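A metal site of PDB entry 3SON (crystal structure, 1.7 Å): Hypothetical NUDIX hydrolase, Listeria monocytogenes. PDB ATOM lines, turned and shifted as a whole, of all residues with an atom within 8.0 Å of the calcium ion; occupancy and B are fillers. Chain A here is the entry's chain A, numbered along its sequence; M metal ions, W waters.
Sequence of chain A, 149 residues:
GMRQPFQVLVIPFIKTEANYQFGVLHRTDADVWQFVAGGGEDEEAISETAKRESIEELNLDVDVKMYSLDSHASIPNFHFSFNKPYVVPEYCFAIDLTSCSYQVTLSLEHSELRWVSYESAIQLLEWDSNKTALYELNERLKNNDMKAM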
ATOM      1  N   GLN A   7      -5.917  16.234   4.346  1.00  0.00           N
ATOM      2  CA  GLN A   7      -7.244  16.531   3.916  1.00  0.00           C
ATOM      3  C   GLN A   7      -7.375  16.350   2.407  1.00  0.00           C
ATOM      4  O   GLN A   7      -6.387  16.408   1.660  1.00  0.00           O
ATOM      5  CB  GLN A   7      -7.558  17.996   4.183  1.00  0.00           C
ATOM      6  CG  GLN A   7      -7.856  18.317   5.642  1.00  0.00           C
ATOM      7  CD  GLN A   7      -9.251  17.916   6.026  1.00  0.00           C
ATOM      8  OE1 GLN A   7     -10.240  18.299   5.382  1.00  0.00           O
ATOM      9  NE2 GLN A   7      -9.343  17.120   7.028  1.00  0.00           N
ATOM     10  N   VAL A   8      -8.569  16.060   1.977  1.00  0.00           N
ATOM     11  CA  VAL A   8      -8.847  16.057   0.579  1.00  0.00           C
ATOM     12  C   VAL A   8      -9.932  17.076   0.228  1.00  0.00           C
ATOM     13  O   VAL A   8     -10.791  17.455   1.093  1.00  0.00           O
ATOM     14  CB  VAL A   8      -9.140  14.635   0.006  1.00  0.00           C
ATOM     15  CG1 VAL A   8      -8.039  13.588   0.381  1.00  0.00           C
ATOM     16  CG2 VAL A   8     -10.508  14.113   0.482  1.00  0.00           C
ATOM     17  N   ARG A  27     -23.817  24.820   2.916  1.00  0.00           N
ATOM     18  CA  ARG A  27     -23.951  24.186   4.213  1.00  0.00           C
ATOM     19  C   ARG A  27     -25.339  24.380   4.906  1.00  0.00           C
ATOM     20  O   ARG A  27     -26.025  25.430   4.784  1.00  0.00           O
ATOM     21  CB  ARG A  27     -22.872  24.666   5.162  1.00  0.00           C
ATOM     22  CG  ARG A  27     -21.479  24.136   4.796  1.00  0.00           C
ATOM     23  CD  ARG A  27     -20.527  24.399   5.962  1.00  0.00           C
ATOM     24  NE  ARG A  27     -20.857  23.638   7.188  1.00  0.00           N
ATOM     25  CZ  ARG A  27     -20.472  22.388   7.393  1.00  0.00           C
ATOM     26  NH1 ARG A  27     -19.821  21.720   6.438  1.00  0.00           N
ATOM     27  NH2 ARG A  27     -20.778  21.767   8.533  1.00  0.00           N
ATOM     28  N   GLN A  34     -19.078  25.361  -0.337  1.00  0.00           N
ATOM     29  CA  GLN A  34     -17.825  24.601  -0.371  1.00  0.00           C
ATOM     30  C   GLN A  34     -17.889  23.395  -1.319  1.00  0.00           C
ATOM     31  O   GLN A  34     -18.955  23.011  -1.866  1.00  0.00           O
ATOM     32  CB  GLN A  34     -17.449  24.067   1.060  1.00  0.00           C
ATOM     33  CG  GLN A  34     -18.509  23.074   1.609  1.00  0.00           C
ATOM     34  CD  GLN A  34     -18.386  22.691   3.090  1.00  0.00           C
ATOM     35  OE1 GLN A  34     -19.313  22.068   3.637  1.00  0.00           O
ATOM     36  NE2 GLN A  34     -17.211  22.971   3.708  1.00  0.00           N
ATOM     37  N   PHE A  35     -16.742  22.776  -1.504  1.00  0.00           N
ATOM     38  CA  PHE A  35     -16.632  21.514  -2.211  1.00  0.00           C
ATOM     39  C   PHE A  35     -16.677  20.322  -1.226  1.00  0.00           C
ATOM     40  O   PHE A  35     -16.914  20.527  -0.036  1.00  0.00           O
ATOM     41  CB  PHE A  35     -15.359  21.495  -3.074  1.00  0.00           C
ATOM     42  CG  PHE A  35     -15.347  22.523  -4.186  1.00  0.00           C
ATOM     43  CD1 PHE A  35     -16.335  22.570  -5.120  1.00  0.00           C
ATOM     44  CD2 PHE A  35     -14.239  23.391  -4.369  1.00  0.00           C
ATOM     45  CE1 PHE A  35     -16.287  23.504  -6.183  1.00  0.00           C
ATOM     46  CE2 PHE A  35     -14.196  24.351  -5.379  1.00  0.00           C
ATOM     47  CZ  PHE A  35     -15.219  24.409  -6.292  1.00  0.00           C
ATOM     48  N   VAL A  36     -16.623  19.117  -1.771  1.00  0.00           N
ATOM     49  CA  VAL A  36     -16.506  17.902  -0.995  1.00  0.00           C
ATOM     50  C   VAL A  36     -15.191  18.003  -0.224  1.00  0.00           C
ATOM     51  O   VAL A  36     -14.160  18.368  -0.781  1.00  0.00           O
ATOM     52  CB  VAL A  36     -16.565  16.653  -1.896  1.00  0.00           C
ATOM     53  CG1 VAL A  36     -16.121  15.364  -1.175  1.00  0.00           C
ATOM     54  CG2 VAL A  36     -17.916  16.454  -2.485  1.00  0.00           C
ATOM     55  N   ALA A  37     -15.196  17.724   1.075  1.00  0.00           N
ATOM     56  CA  ALA A  37     -13.943  17.850   1.866  1.00  0.00           C
ATOM     57  C   ALA A  37     -13.935  16.833   2.977  1.00  0.00           C
ATOM     58  O   ALA A  37     -14.998  16.523   3.554  1.00  0.00           O
ATOM     59  CB  ALA A  37     -13.811  19.267   2.457  1.00  0.00           C
ATOM     60  N   GLY A  38     -12.763  16.349   3.337  1.00  0.00           N
ATOM     61  CA  GLY A  38     -12.681  15.445   4.466  1.00  0.00           C
ATOM     62  C   GLY A  38     -11.273  15.057   4.781  1.00  0.00           C
ATOM     63  O   GLY A  38     -10.403  15.165   3.935  1.00  0.00           O
ATOM     64  N   GLY A  39     -11.065  14.405   5.908  1.00  0.00           N
ATOM     65  CA  GLY A  39      -9.742  14.011   6.291  1.00  0.00           C
ATOM     66  C   GLY A  39      -9.464  12.521   6.122  1.00  0.00           C
ATOM     67  O   GLY A  39     -10.385  11.677   6.101  1.00  0.00           O
ATOM     68  N   GLU A  41      -8.503   8.879   7.036  1.00  0.00           N
ATOM     69  CA  GLU A  41      -8.710   7.990   8.193  1.00  0.00           C
ATOM     70  C   GLU A  41      -7.881   6.726   8.094  1.00  0.00           C
ATOM     71  O   GLU A  41      -7.531   6.294   6.998  1.00  0.00           O
ATOM     72  CB  GLU A  41     -10.200   7.604   8.281  1.00  0.00           C
ATOM     73  CG  GLU A  41     -11.084   8.799   8.575  1.00  0.00           C
ATOM     74  CD  GLU A  41     -12.560   8.433   8.626  1.00  0.00           C
ATOM     75  OE1 GLU A  41     -12.862   7.229   8.688  1.00  0.00           O
ATOM     76  OE2 GLU A  41     -13.405   9.355   8.544  1.00  0.00           O
ATOM     77  N   THR A  49      -9.353   8.105   0.436  1.00  0.00           N
ATOM     78  CA  THR A  49     -10.080   9.189   1.177  1.00  0.00           C
ATOM     79  C   THR A  49     -10.960   9.990   0.230  1.00  0.00           C
ATOM     80  O   THR A  49     -12.110  10.268   0.550  1.00  0.00           O
ATOM     81  CB  THR A  49      -9.088  10.133   1.874  1.00  0.00           C
ATOM     82  OG1 THR A  49      -8.174   9.351   2.615  1.00  0.00           O
ATOM     83  CG2 THR A  49      -9.849  11.123   2.850  1.00  0.00           C
ATOM     84  N   ARG A  52     -13.994   7.876  -0.752  1.00  0.00           N
ATOM     85  CA  ARG A  52     -14.888   7.701   0.406  1.00  0.00           C
ATOM     86  C   ARG A  52     -15.701   8.951   0.685  1.00  0.00           C
ATOM     87  O   ARG A  52     -16.922   8.839   0.889  1.00  0.00           O
ATOM     88  CB  ARG A  52     -14.116   7.297   1.656  1.00  0.00           C
ATOM     89  CG  ARG A  52     -15.040   6.991   2.865  1.00  0.00           C
ATOM     90  CD  ARG A  52     -14.281   6.577   4.163  1.00  0.00           C
ATOM     91  NE  ARG A  52     -13.081   7.399   4.377  1.00  0.00           N
ATOM     92  CZ  ARG A  52     -13.101   8.660   4.796  1.00  0.00           C
ATOM     93  NH1 ARG A  52     -14.257   9.265   5.125  1.00  0.00           N
ATOM     94  NH2 ARG A  52     -11.943   9.337   4.896  1.00  0.00           N
ATOM     95  N   GLU A  53     -15.024  10.109   0.688  1.00  0.00           N
ATOM     96  CA  GLU A  53     -15.675  11.377   1.050  1.00  0.00           C
ATOM     97  C   GLU A  53     -16.700  11.754  -0.007  1.00  0.00           C
ATOM     98  O   GLU A  53     -17.757  12.320   0.310  1.00  0.00           O
ATOM     99  CB  GLU A  53     -14.657  12.488   1.226  1.00  0.00           C
ATOM    100  CG  GLU A  53     -13.816  12.280   2.461  1.00  0.00           C
ATOM    101  CD  GLU A  53     -14.584  12.551   3.786  1.00  0.00           C
ATOM    102  OE1 GLU A  53     -15.582  13.288   3.754  1.00  0.00           O
ATOM    103  OE2 GLU A  53     -14.106  12.072   4.853  1.00  0.00           O
ATOM    104  N   SER A  54     -16.340  11.511  -1.258  1.00  0.00           N
ATOM    105  CA  SER A  54     -17.234  11.746  -2.371  1.00  0.00           C
ATOM    106  C   SER A  54     -18.469  10.872  -2.247  1.00  0.00           C
ATOM    107  O   SER A  54     -19.592  11.346  -2.444  1.00  0.00           O
ATOM    108  CB  SER A  54     -16.498  11.486  -3.712  1.00  0.00           C
ATOM    109  OG  SER A  54     -15.462  12.463  -3.833  1.00  0.00           O
ATOM    110  N   GLU A  56     -19.670   9.551   0.617  1.00  0.00           N
ATOM    111  CA  GLU A  56     -20.400   9.938   1.783  1.00  0.00           C
ATOM    112  C   GLU A  56     -21.228  11.203   1.469  1.00  0.00           C
ATOM    113  O   GLU A  56     -22.406  11.271   1.777  1.00  0.00           O
ATOM    114  CB  GLU A  56     -19.462  10.211   2.987  1.00  0.00           C
ATOM    115  CG  GLU A  56     -18.693   8.984   3.507  1.00  0.00           C
ATOM    116  CD  GLU A  56     -17.761   9.280   4.711  1.00  0.00           C
ATOM    117  OE1 GLU A  56     -17.571  10.487   5.039  1.00  0.00           O
ATOM    118  OE2 GLU A  56     -17.223   8.307   5.339  1.00  0.00           O
ATOM    119  N   GLU A  57     -20.613  12.176   0.823  1.00  0.00           N
ATOM    120  CA  GLU A  57     -21.298  13.456   0.672  1.00  0.00           C
ATOM    121  C   GLU A  57     -22.349  13.499  -0.431  1.00  0.00           C
ATOM    122  O   GLU A  57     -23.296  14.287  -0.333  1.00  0.00           O
ATOM    123  CB  GLU A  57     -20.290  14.597   0.496  1.00  0.00           C
ATOM    124  CG  GLU A  57     -19.382  14.785   1.720  1.00  0.00           C
ATOM    125  CD  GLU A  57     -18.672  16.111   1.717  1.00  0.00           C
ATOM    126  OE1 GLU A  57     -19.145  17.059   1.030  1.00  0.00           O
ATOM    127  OE2 GLU A  57     -17.616  16.228   2.392  1.00  0.00           O
ATOM    128  N   SER A 107     -26.045  14.571   2.113  1.00  0.00           N
ATOM    129  CA  SER A 107     -26.123  14.279   3.532  1.00  0.00           C
ATOM    130  C   SER A 107     -26.705  15.472   4.271  1.00  0.00           C
ATOM    131  O   SER A 107     -26.892  16.571   3.694  1.00  0.00           O
ATOM    132  CB  SER A 107     -24.749  13.925   4.101  1.00  0.00           C
ATOM    133  OG  SER A 107     -23.909  15.044   4.238  1.00  0.00           O
ATOM    134  N   GLU A 109     -25.375  17.510   6.177  1.00  0.00           N
ATOM    135  CA  GLU A 109     -24.421  18.613   6.318  1.00  0.00           C
ATOM    136  C   GLU A 109     -24.698  19.753   5.319  1.00  0.00           C
ATOM    137  O   GLU A 109     -24.274  20.853   5.580  1.00  0.00           O
ATOM    138  CB  GLU A 109     -22.990  18.081   6.063  1.00  0.00           C
ATOM    139  CG  GLU A 109     -21.919  19.015   6.640  1.00  0.00           C
ATOM    140  CD  GLU A 109     -20.547  18.352   6.746  1.00  0.00           C
ATOM    141  OE1 GLU A 109     -20.419  17.356   7.492  1.00  0.00           O
ATOM    142  OE2 GLU A 109     -19.611  18.841   6.080  1.00  0.00           O
ATOM    143  N   HIS A 110     -25.417  19.449   4.235  1.00  0.00           N
ATOM    144  CA  HIS A 110     -25.674  20.374   3.131  1.00  0.00           C
ATOM    145  C   HIS A 110     -27.122  20.573   2.785  1.00  0.00           C
ATOM    146  O   HIS A 110     -27.970  19.654   2.917  1.00  0.00           O
ATOM    147  CB  HIS A 110     -24.885  19.902   1.856  1.00  0.00           C
ATOM    148  CG  HIS A 110     -23.400  19.863   2.079  1.00  0.00           C
ATOM    149  ND1 HIS A 110     -22.722  18.715   2.070  1.00  0.00           N
ATOM    150  CD2 HIS A 110     -22.490  20.843   2.376  1.00  0.00           C
ATOM    151  CE1 HIS A 110     -21.449  18.947   2.357  1.00  0.00           C
ATOM    152  NE2 HIS A 110     -21.302  20.233   2.554  1.00  0.00           N
HETATM  153 CA    CA M   1     -16.591  15.214   4.616  1.00  0.00          CA
HETATM  154  O   HOH W   1     -15.491  16.675   6.560  1.00  0.00           O
HETATM  155  O   HOH W   2     -17.323  13.532   5.733  1.00  0.00           O
HETATM  156  O   HOH W   3     -14.583  13.917   6.921  1.00  0.00           O
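The side-chain carboxylate (OE2) of Glu 53 lies within salt-bridge range of the guanidinium group (NH1) of Arg 52, 2.8 Å away.
The backbone carbonyl oxygen of Gly 38 is in hydrogen-bond range of the backbone NH of Val 8 (2.8 Å).
The backbone carbonyl oxygen of Gly 38 lies close to the side-chain amide oxygen of Gln 7 (3.5 Å).
The calcium ion is bound by water W2.
O of Ala 37 binds the calcium ion (2.3 Å).
The side-chain carboxylate (OE1) of Glu 53 binds the calcium ion, 2.3 Å away.
The side-chain carboxylate (OE2) of Glu 57 is bound to the calcium ion (2.7 Å).
Water W1 is bound to the calcium ion.
Gly 38 touches the calcium ion.
Four residues have an atom within 4 Å of the calcium ion: Ala 37, Gly 38, Glu 53 and Glu 57.
The nearest printed residue that does not touch the calcium ion is Glu 56 (4.8 Å).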
